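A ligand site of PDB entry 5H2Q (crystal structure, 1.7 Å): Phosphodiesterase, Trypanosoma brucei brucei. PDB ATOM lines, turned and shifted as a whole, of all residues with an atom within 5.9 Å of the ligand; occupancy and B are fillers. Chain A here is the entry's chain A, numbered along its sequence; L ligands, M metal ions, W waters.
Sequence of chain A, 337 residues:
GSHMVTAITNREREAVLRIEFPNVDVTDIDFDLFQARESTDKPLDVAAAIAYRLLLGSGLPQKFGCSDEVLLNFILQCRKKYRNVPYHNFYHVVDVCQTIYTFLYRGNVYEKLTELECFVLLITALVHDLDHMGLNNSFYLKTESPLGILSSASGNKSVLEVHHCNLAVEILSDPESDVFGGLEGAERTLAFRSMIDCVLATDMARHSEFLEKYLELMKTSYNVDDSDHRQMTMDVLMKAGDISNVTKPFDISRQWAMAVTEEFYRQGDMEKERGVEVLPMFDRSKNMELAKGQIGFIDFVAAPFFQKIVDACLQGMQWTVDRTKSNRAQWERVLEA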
ATOM      1  N   TYR A  87      -5.048  14.212 -21.009  1.00  0.00           N
ATOM      2  CA  TYR A  87      -4.908  12.834 -20.502  1.00  0.00           C
ATOM      3  C   TYR A  87      -5.701  12.547 -19.239  1.00  0.00           C
ATOM      4  O   TYR A  87      -6.442  11.582 -19.220  1.00  0.00           O
ATOM      5  CB  TYR A  87      -3.434  12.457 -20.307  1.00  0.00           C
ATOM      6  CG  TYR A  87      -3.215  11.016 -19.868  1.00  0.00           C
ATOM      7  CD1 TYR A  87      -3.160   9.976 -20.806  1.00  0.00           C
ATOM      8  CD2 TYR A  87      -3.171  10.674 -18.518  1.00  0.00           C
ATOM      9  CE1 TYR A  87      -2.954   8.657 -20.405  1.00  0.00           C
ATOM     10  CE2 TYR A  87      -2.989   9.349 -18.111  1.00  0.00           C
ATOM     11  CZ  TYR A  87      -2.884   8.344 -19.056  1.00  0.00           C
ATOM     12  OH  TYR A  87      -2.755   7.042 -18.616  1.00  0.00           O
ATOM     13  N   HIS A  88      -5.530  13.364 -18.179  1.00  0.00           N
ATOM     14  CA  HIS A  88      -6.202  13.114 -16.916  1.00  0.00           C
ATOM     15  C   HIS A  88      -7.630  13.646 -16.896  1.00  0.00           C
ATOM     16  O   HIS A  88      -8.031  14.406 -16.014  1.00  0.00           O
ATOM     17  CB  HIS A  88      -5.367  13.615 -15.731  1.00  0.00           C
ATOM     18  CG  HIS A  88      -4.153  12.773 -15.442  1.00  0.00           C
ATOM     19  ND1 HIS A  88      -2.896  13.172 -15.832  1.00  0.00           N
ATOM     20  CD2 HIS A  88      -4.064  11.569 -14.837  1.00  0.00           C
ATOM     21  CE1 HIS A  88      -2.075  12.207 -15.452  1.00  0.00           C
ATOM     22  NE2 HIS A  88      -2.727  11.234 -14.807  1.00  0.00           N
ATOM     23  N   HIS A 132      -7.885  16.509 -11.376  1.00  0.00           N
ATOM     24  CA  HIS A 132      -6.533  16.636 -11.954  1.00  0.00           C
ATOM     25  C   HIS A 132      -6.606  17.800 -12.941  1.00  0.00           C
ATOM     26  O   HIS A 132      -7.633  17.989 -13.598  1.00  0.00           O
ATOM     27  CB  HIS A 132      -6.139  15.340 -12.656  1.00  0.00           C
ATOM     28  CG  HIS A 132      -4.659  15.113 -12.737  1.00  0.00           C
ATOM     29  ND1 HIS A 132      -3.873  15.844 -13.621  1.00  0.00           N
ATOM     30  CD2 HIS A 132      -3.878  14.236 -12.071  1.00  0.00           C
ATOM     31  CE1 HIS A 132      -2.634  15.414 -13.431  1.00  0.00           C
ATOM     32  NE2 HIS A 132      -2.598  14.420 -12.522  1.00  0.00           N
ATOM     33  N   THR A 202      -1.161   5.442  -5.823  1.00  0.00           N
ATOM     34  CA  THR A 202      -0.975   5.856  -7.207  1.00  0.00           C
ATOM     35  C   THR A 202       0.110   6.917  -7.409  1.00  0.00           C
ATOM     36  O   THR A 202       0.375   7.264  -8.560  1.00  0.00           O
ATOM     37  CB  THR A 202      -2.288   6.273  -7.864  1.00  0.00           C
ATOM     38  OG1 THR A 202      -2.733   7.451  -7.218  1.00  0.00           O
ATOM     39  CG2 THR A 202      -3.335   5.158  -7.830  1.00  0.00           C
ATOM     40  N   MET A 204       3.392   8.009  -8.248  1.00  0.00           N
ATOM     41  CA  MET A 204       4.520   7.314  -8.902  1.00  0.00           C
ATOM     42  C   MET A 204       5.893   7.555  -8.231  1.00  0.00           C
ATOM     43  O   MET A 204       6.819   6.761  -8.450  1.00  0.00           O
ATOM     44  CB  MET A 204       4.611   7.595 -10.392  1.00  0.00           C
ATOM     45  CG  MET A 204       3.530   6.939 -11.213  1.00  0.00           C
ATOM     46  SD  MET A 204       3.562   5.129 -11.096  1.00  0.00           S
ATOM     47  CE  MET A 204       5.003   4.707 -12.033  1.00  0.00           C
ATOM     48  N   ASP A 242      -3.372   2.052 -13.638  1.00  0.00           N
ATOM     49  CA  ASP A 242      -2.805   3.377 -13.943  1.00  0.00           C
ATOM     50  C   ASP A 242      -1.718   3.339 -15.005  1.00  0.00           C
ATOM     51  O   ASP A 242      -1.629   4.261 -15.807  1.00  0.00           O
ATOM     52  CB  ASP A 242      -2.271   4.012 -12.672  1.00  0.00           C
ATOM     53  CG  ASP A 242      -2.843   5.381 -12.369  1.00  0.00           C
ATOM     54  OD1 ASP A 242      -3.524   5.965 -13.270  1.00  0.00           O
ATOM     55  OD2 ASP A 242      -2.516   5.916 -11.296  1.00  0.00           O
ATOM     56  N   ILE A 243      -0.908   2.262 -15.026  1.00  0.00           N
ATOM     57  CA  ILE A 243       0.172   2.152 -16.006  1.00  0.00           C
ATOM     58  C   ILE A 243      -0.135   1.104 -17.102  1.00  0.00           C
ATOM     59  O   ILE A 243       0.768   0.633 -17.792  1.00  0.00           O
ATOM     60  CB  ILE A 243       1.560   1.953 -15.358  1.00  0.00           C
ATOM     61  CG1 ILE A 243       1.693   0.603 -14.593  1.00  0.00           C
ATOM     62  CG2 ILE A 243       1.932   3.153 -14.480  1.00  0.00           C
ATOM     63  CD1 ILE A 243       3.204   0.354 -14.048  1.00  0.00           C
ATOM     64  N   ASN A 245      -1.761   1.484 -20.070  1.00  0.00           N
ATOM     65  CA  ASN A 245      -1.898   1.912 -21.480  1.00  0.00           C
ATOM     66  C   ASN A 245      -0.928   1.152 -22.393  1.00  0.00           C
ATOM     67  O   ASN A 245      -1.246   0.907 -23.555  1.00  0.00           O
ATOM     68  CB  ASN A 245      -1.650   3.416 -21.641  1.00  0.00           C
ATOM     69  CG  ASN A 245      -2.546   4.363 -20.878  1.00  0.00           C
ATOM     70  OD1 ASN A 245      -2.128   5.502 -20.613  1.00  0.00           O
ATOM     71  ND2 ASN A 245      -3.783   3.971 -20.539  1.00  0.00           N
ATOM     72  N   VAL A 246       0.231   0.766 -21.861  1.00  0.00           N
ATOM     73  CA  VAL A 246       1.236   0.018 -22.650  1.00  0.00           C
ATOM     74  C   VAL A 246       0.839  -1.455 -22.902  1.00  0.00           C
ATOM     75  O   VAL A 246       1.488  -2.103 -23.727  1.00  0.00           O
ATOM     76  CB  VAL A 246       2.652   0.135 -22.029  1.00  0.00           C
ATOM     77  CG1 VAL A 246       3.077   1.592 -21.916  1.00  0.00           C
ATOM     78  CG2 VAL A 246       2.708  -0.549 -20.667  1.00  0.00           C
ATOM     79  N   SER A 253      -2.801   1.946 -27.450  1.00  0.00           N
ATOM     80  CA  SER A 253      -1.589   2.313 -26.695  1.00  0.00           C
ATOM     81  C   SER A 253      -0.976   3.600 -27.267  1.00  0.00           C
ATOM     82  O   SER A 253      -0.630   4.506 -26.496  1.00  0.00           O
ATOM     83  CB  SER A 253      -0.571   1.178 -26.741  1.00  0.00           C
ATOM     84  OG  SER A 253       0.420   1.362 -25.748  1.00  0.00           O
ATOM     85  N   TRP A 256      -3.127   6.704 -26.345  1.00  0.00           N
ATOM     86  CA  TRP A 256      -2.866   7.091 -24.959  1.00  0.00           C
ATOM     87  C   TRP A 256      -1.523   7.863 -24.883  1.00  0.00           C
ATOM     88  O   TRP A 256      -1.452   8.874 -24.182  1.00  0.00           O
ATOM     89  CB  TRP A 256      -2.801   5.864 -24.043  1.00  0.00           C
ATOM     90  CG  TRP A 256      -4.130   5.227 -23.767  1.00  0.00           C
ATOM     91  CD1 TRP A 256      -4.505   3.938 -24.042  1.00  0.00           C
ATOM     92  CD2 TRP A 256      -5.287   5.850 -23.186  1.00  0.00           C
ATOM     93  NE1 TRP A 256      -5.791   3.717 -23.646  1.00  0.00           N
ATOM     94  CE2 TRP A 256      -6.308   4.876 -23.120  1.00  0.00           C
ATOM     95  CE3 TRP A 256      -5.553   7.144 -22.707  1.00  0.00           C
ATOM     96  CZ2 TRP A 256      -7.580   5.166 -22.628  1.00  0.00           C
ATOM     97  CZ3 TRP A 256      -6.819   7.428 -22.210  1.00  0.00           C
ATOM     98  CH2 TRP A 256      -7.803   6.433 -22.140  1.00  0.00           C
ATOM     99  N   ALA A 257      -0.496   7.398 -25.607  1.00  0.00           N
ATOM    100  CA  ALA A 257       0.827   8.019 -25.676  1.00  0.00           C
ATOM    101  C   ALA A 257       0.734   9.434 -26.235  1.00  0.00           C
ATOM    102  O   ALA A 257       1.318  10.358 -25.663  1.00  0.00           O
ATOM    103  CB  ALA A 257       1.772   7.176 -26.519  1.00  0.00           C
ATOM    104  N   VAL A 260      -0.985  11.644 -23.364  1.00  0.00           N
ATOM    105  CA  VAL A 260      -0.065  11.925 -22.256  1.00  0.00           C
ATOM    106  C   VAL A 260       1.019  12.939 -22.680  1.00  0.00           C
ATOM    107  O   VAL A 260       1.341  13.852 -21.907  1.00  0.00           O
ATOM    108  CB  VAL A 260       0.532  10.672 -21.566  1.00  0.00           C
ATOM    109  CG1 VAL A 260       1.708  10.066 -22.350  1.00  0.00           C
ATOM    110  CG2 VAL A 260       0.959  11.000 -20.130  1.00  0.00           C
ATOM    111  N   THR A 261       1.541  12.782 -23.902  1.00  0.00           N
ATOM    112  CA  THR A 261       2.555  13.691 -24.487  1.00  0.00           C
ATOM    113  C   THR A 261       2.021  15.110 -24.531  1.00  0.00           C
ATOM    114  O   THR A 261       2.693  16.004 -24.013  1.00  0.00           O
ATOM    115  CB  THR A 261       2.983  13.178 -25.880  1.00  0.00           C
ATOM    116  OG1 THR A 261       3.589  11.915 -25.700  1.00  0.00           O
ATOM    117  CG2 THR A 261       3.985  14.123 -26.575  1.00  0.00           C
ATOM    118  N   PHE A 264       1.703  16.532 -20.962  1.00  0.00           N
ATOM    119  CA  PHE A 264       3.042  16.788 -20.422  1.00  0.00           C
ATOM    120  C   PHE A 264       3.646  18.054 -21.044  1.00  0.00           C
ATOM    121  O   PHE A 264       4.151  18.905 -20.312  1.00  0.00           O
ATOM    122  CB  PHE A 264       3.957  15.566 -20.621  1.00  0.00           C
ATOM    123  CG  PHE A 264       3.813  14.456 -19.599  1.00  0.00           C
ATOM    124  CD1 PHE A 264       2.695  14.378 -18.770  1.00  0.00           C
ATOM    125  CD2 PHE A 264       4.779  13.457 -19.504  1.00  0.00           C
ATOM    126  CE1 PHE A 264       2.558  13.328 -17.849  1.00  0.00           C
ATOM    127  CE2 PHE A 264       4.650  12.427 -18.565  1.00  0.00           C
ATOM    128  CZ  PHE A 264       3.542  12.367 -17.749  1.00  0.00           C
ATOM    129  N   TYR A 265       3.477  18.227 -22.369  1.00  0.00           N
ATOM    130  CA  TYR A 265       3.980  19.406 -23.090  1.00  0.00           C
ATOM    131  C   TYR A 265       3.301  20.689 -22.620  1.00  0.00           C
ATOM    132  O   TYR A 265       3.961  21.732 -22.544  1.00  0.00           O
ATOM    133  CB  TYR A 265       3.796  19.217 -24.607  1.00  0.00           C
ATOM    134  CG  TYR A 265       4.799  18.283 -25.249  1.00  0.00           C
ATOM    135  CD1 TYR A 265       5.862  17.761 -24.522  1.00  0.00           C
ATOM    136  CD2 TYR A 265       4.694  17.930 -26.592  1.00  0.00           C
ATOM    137  CE1 TYR A 265       6.825  16.949 -25.122  1.00  0.00           C
ATOM    138  CE2 TYR A 265       5.643  17.116 -27.196  1.00  0.00           C
ATOM    139  CZ  TYR A 265       6.694  16.619 -26.458  1.00  0.00           C
ATOM    140  OH  TYR A 265       7.613  15.779 -27.051  1.00  0.00           O
ATOM    141  N   MET A 281      11.072  15.523 -20.761  1.00  0.00           N
ATOM    142  CA  MET A 281       9.818  14.811 -21.066  1.00  0.00           C
ATOM    143  C   MET A 281       8.627  15.772 -21.274  1.00  0.00           C
ATOM    144  O   MET A 281       7.659  15.412 -21.955  1.00  0.00           O
ATOM    145  CB  MET A 281       9.516  13.896 -19.872  1.00  0.00           C
ATOM    146  CG  MET A 281       8.692  12.725 -20.225  1.00  0.00           C
ATOM    147  SD  MET A 281       8.324  11.742 -18.773  1.00  0.00           S
ATOM    148  CE  MET A 281       9.675  10.554 -18.855  1.00  0.00           C
ATOM    149  N   PHE A 282       8.696  16.973 -20.680  1.00  0.00           N
ATOM    150  CA  PHE A 282       7.642  18.003 -20.721  1.00  0.00           C
ATOM    151  C   PHE A 282       7.940  19.189 -21.680  1.00  0.00           C
ATOM    152  O   PHE A 282       7.129  20.098 -21.785  1.00  0.00           O
ATOM    153  CB  PHE A 282       7.375  18.517 -19.275  1.00  0.00           C
ATOM    154  CG  PHE A 282       7.089  17.445 -18.248  1.00  0.00           C
ATOM    155  CD1 PHE A 282       8.113  16.735 -17.639  1.00  0.00           C
ATOM    156  CD2 PHE A 282       5.775  17.139 -17.889  1.00  0.00           C
ATOM    157  CE1 PHE A 282       7.855  15.744 -16.692  1.00  0.00           C
ATOM    158  CE2 PHE A 282       5.514  16.151 -16.932  1.00  0.00           C
ATOM    159  CZ  PHE A 282       6.546  15.447 -16.356  1.00  0.00           C
ATOM    160  N   LEU A 290       8.063  10.109 -29.979  1.00  0.00           N
ATOM    161  CA  LEU A 290       7.026   9.447 -29.190  1.00  0.00           C
ATOM    162  C   LEU A 290       7.483   8.014 -28.830  1.00  0.00           C
ATOM    163  O   LEU A 290       7.381   7.610 -27.673  1.00  0.00           O
ATOM    164  CB  LEU A 290       5.707   9.426 -29.994  1.00  0.00           C
ATOM    165  CG  LEU A 290       4.425   8.923 -29.294  1.00  0.00           C
ATOM    166  CD1 LEU A 290       4.070   9.785 -28.096  1.00  0.00           C
ATOM    167  CD2 LEU A 290       3.259   8.917 -30.254  1.00  0.00           C
ATOM    168  N   LYS A 292      10.616   6.783 -28.547  1.00  0.00           N
ATOM    169  CA  LYS A 292      11.674   6.823 -27.517  1.00  0.00           C
ATOM    170  C   LYS A 292      11.064   6.958 -26.109  1.00  0.00           C
ATOM    171  O   LYS A 292      11.504   6.271 -25.180  1.00  0.00           O
ATOM    172  CB  LYS A 292      12.625   8.007 -27.778  1.00  0.00           C
ATOM    173  CG  LYS A 292      13.649   7.740 -28.868  1.00  0.00           C
ATOM    174  CD  LYS A 292      14.358   9.009 -29.323  1.00  0.00           C
ATOM    175  CE  LYS A 292      15.292   8.728 -30.466  1.00  0.00           C
ATOM    176  NZ  LYS A 292      15.646   9.964 -31.220  1.00  0.00           N
ATOM    177  N   GLY A 293      10.058   7.824 -25.974  1.00  0.00           N
ATOM    178  CA  GLY A 293       9.367   8.058 -24.712  1.00  0.00           C
ATOM    179  C   GLY A 293       8.691   6.802 -24.187  1.00  0.00           C
ATOM    180  O   GLY A 293       8.890   6.404 -23.037  1.00  0.00           O
ATOM    181  N   GLN A 294       7.972   6.119 -25.076  1.00  0.00           N
ATOM    182  CA  GLN A 294       7.271   4.867 -24.719  1.00  0.00           C
ATOM    183  C   GLN A 294       8.229   3.718 -24.370  1.00  0.00           C
ATOM    184  O   GLN A 294       8.001   2.988 -23.380  1.00  0.00           O
ATOM    185  CB  GLN A 294       6.260   4.480 -25.811  1.00  0.00           C
ATOM    186  CG  GLN A 294       5.034   5.410 -25.838  1.00  0.00           C
ATOM    187  CD  GLN A 294       4.216   5.339 -24.567  1.00  0.00           C
ATOM    188  OE1 GLN A 294       3.525   4.350 -24.292  1.00  0.00           O
ATOM    189  NE2 GLN A 294       4.285   6.369 -23.743  1.00  0.00           N
ATOM    190  N   PHE A 297       9.601   4.390 -20.841  1.00  0.00           N
ATOM    191  CA  PHE A 297       8.506   4.116 -19.897  1.00  0.00           C
ATOM    192  C   PHE A 297       8.342   2.603 -19.690  1.00  0.00           C
ATOM    193  O   PHE A 297       8.311   2.145 -18.542  1.00  0.00           O
ATOM    194  CB  PHE A 297       7.200   4.765 -20.381  1.00  0.00           C
ATOM    195  CG  PHE A 297       6.046   4.615 -19.413  1.00  0.00           C
ATOM    196  CD1 PHE A 297       6.138   5.104 -18.111  1.00  0.00           C
ATOM    197  CD2 PHE A 297       4.856   4.005 -19.804  1.00  0.00           C
ATOM    198  CE1 PHE A 297       5.075   4.949 -17.213  1.00  0.00           C
ATOM    199  CE2 PHE A 297       3.800   3.857 -18.907  1.00  0.00           C
ATOM    200  CZ  PHE A 297       3.910   4.342 -17.620  1.00  0.00           C
ATOM    201  N   VAL A 301       9.891   1.322 -16.212  1.00  0.00           N
ATOM    202  CA  VAL A 301       8.704   1.297 -15.351  1.00  0.00           C
ATOM    203  C   VAL A 301       7.778   0.074 -15.598  1.00  0.00           C
ATOM    204  O   VAL A 301       7.725  -0.811 -14.744  1.00  0.00           O
ATOM    205  CB  VAL A 301       7.905   2.637 -15.358  1.00  0.00           C
ATOM    206  CG1 VAL A 301       6.718   2.586 -14.405  1.00  0.00           C
ATOM    207  CG2 VAL A 301       8.795   3.828 -15.015  1.00  0.00           C
HETATM  208  C1  LIG L   1       3.423   7.556 -19.910  1.00  0.00           C
HETATM  209  C2  LIG L   1       2.191   7.079 -20.403  1.00  0.00           C
HETATM  210  O1  LIG L   1       4.422   7.701 -20.843  1.00  0.00           O
HETATM  211  C3  LIG L   1       1.381   8.281 -15.360  1.00  0.00           C
HETATM  212  C4  LIG L   1       1.561   9.498 -14.420  1.00  0.00           C
HETATM  213  C5  LIG L   1       2.952   9.569 -13.803  1.00  0.00           C
HETATM  214  C6  LIG L   1       1.439   6.960 -14.569  1.00  0.00           C
HETATM  215  C7  LIG L   1       0.646   7.017 -13.284  1.00  0.00           C
HETATM  216  C8  LIG L   1       0.464   9.504 -13.340  1.00  0.00           C
HETATM  217  C9  LIG L   1       0.317   8.154 -12.681  1.00  0.00           C
HETATM  218  C10 LIG L   1       5.377   9.131 -14.282  1.00  0.00           C
HETATM  219  C11 LIG L   1       6.158  10.096 -15.244  1.00  0.00           C
HETATM  220  C12 LIG L   1       5.934   7.676 -14.264  1.00  0.00           C
HETATM  221  C13 LIG L   1       7.658  10.302 -14.990  1.00  0.00           C
HETATM  222  C14 LIG L   1       7.393   7.442 -13.898  1.00  0.00           C
HETATM  223  C15 LIG L   1       8.408   7.759 -15.004  1.00  0.00           C
HETATM  224  C16 LIG L   1       8.585   9.197 -15.508  1.00  0.00           C
HETATM  225  C17 LIG L   1       5.706   8.157 -20.373  1.00  0.00           C
HETATM  226  C18 LIG L   1       6.577   8.331 -21.594  1.00  0.00           C
HETATM  227  C19 LIG L   1       3.531   7.948 -18.587  1.00  0.00           C
HETATM  228  C20 LIG L   1       1.082   7.034 -19.559  1.00  0.00           C
HETATM  229  C21 LIG L   1       2.422   7.889 -17.739  1.00  0.00           C
HETATM  230  C22 LIG L   1       1.203   7.440 -18.237  1.00  0.00           C
HETATM  231  O2  LIG L   1       2.181   6.678 -21.708  1.00  0.00           O
HETATM  232  C23 LIG L   1       0.922   6.413 -22.332  1.00  0.00           C
HETATM  233  C24 LIG L   1       2.556   8.328 -16.326  1.00  0.00           C
HETATM  234  N1  LIG L   1       3.754   8.751 -15.977  1.00  0.00           N
HETATM  235  N2  LIG L   1       3.947   9.158 -14.679  1.00  0.00           N
HETATM  236  O3  LIG L   1       3.148   9.942 -12.655  1.00  0.00           O
HETATM  237  N3  LIG L   1       6.301   9.582 -22.316  1.00  0.00           N
HETATM  238  C25 LIG L   1       6.110  10.867 -21.633  1.00  0.00           C
HETATM  239  C26 LIG L   1       5.832   9.641 -23.603  1.00  0.00           C
HETATM  240  C27 LIG L   1       5.816  11.820 -22.791  1.00  0.00           C
HETATM  241  N4  LIG L   1       5.542  10.919 -23.887  1.00  0.00           N
HETATM  242  O4  LIG L   1       5.748   8.682 -24.355  1.00  0.00           O
HETATM  243 MG    MG M   1      -3.004  10.189 -10.346  1.00  0.00          MG
HETATM  244 ZN    ZN M   2      -4.548   7.852 -13.081  1.00  0.00          ZN
HETATM  245  O   HOH W   1      -2.011  10.908 -12.009  1.00  0.00           O
HETATM  246  O   HOH W   2       0.680   3.693 -24.080  1.00  0.00           O
HETATM  247  O   HOH W   3       1.932   9.813 -10.220  1.00  0.00           O
HETATM  248  O   HOH W   4      -2.762   8.600 -14.092  1.00  0.00           O
HETATM  249  O   HOH W   5      -1.652   6.966 -15.978  1.00  0.00           O
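A nitrogen (N4) of the ligand lies within hydrogen-bond range of the side-chain hydroxyl (OG1) of Thr 261, 2.8 Å away. An oxygen (O4) of the ligand lies within hydrogen-bond range of the backbone NH of Gln 294. NE2 of Gln 294 sits at hydrogen-bond distance from O4 of the ligand, at 2.8 Å.
OD1 of Asn 245 lies within hydrogen-bond range of OH of Tyr 87 (2.6 Å). The side-chain hydroxyl of Ser 253 sits at hydrogen-bond distance from the backbone carbonyl oxygen of Asn 245. OG1 of Thr 261 is in hydrogen-bond range of O of Ala 257.
Tyr 87 touches the ligand. His 88 touches the ligand. Met 204 touches the ligand. OD2 of Asp 242 touches C9 of the ligand, at 3.9 Å. Ile 243 touches the ligand. Asn 245 touches the ligand (OD1 to C23, 3.6 Å). Trp 256 touches the ligand (C to C23, 3.8 Å). N of Ala 257 touches C23 of the ligand, 3.7 Å away. CG1 of Val 260 touches O2 of the ligand, at 3.5 Å. Phe 264 touches the ligand. Met 281 touches the ligand (CG to C25, 3.5 Å). Leu 290 touches the ligand (O to O4, 3.9 Å). O of Gly 293 touches C18 of the ligand, 3.3 Å away. Phe 297 touches the ligand. CG2 of Val 301 touches C15 of the ligand, 3.95 Å away. Along chain A the residues within 4 Å of the ligand span positions 87 to 301. The nearest printed residue that does not touch the ligand is Thr 202 (4.2 Å).
Water W3 lies within hydrogen-bond range of an oxygen (O3) of the ligand, the backbone NH of Met 204 and the backbone carbonyl oxygen of Thr 202. Water W5 lies within hydrogen-bond range of O of Asp 242 and OH of Tyr 87.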
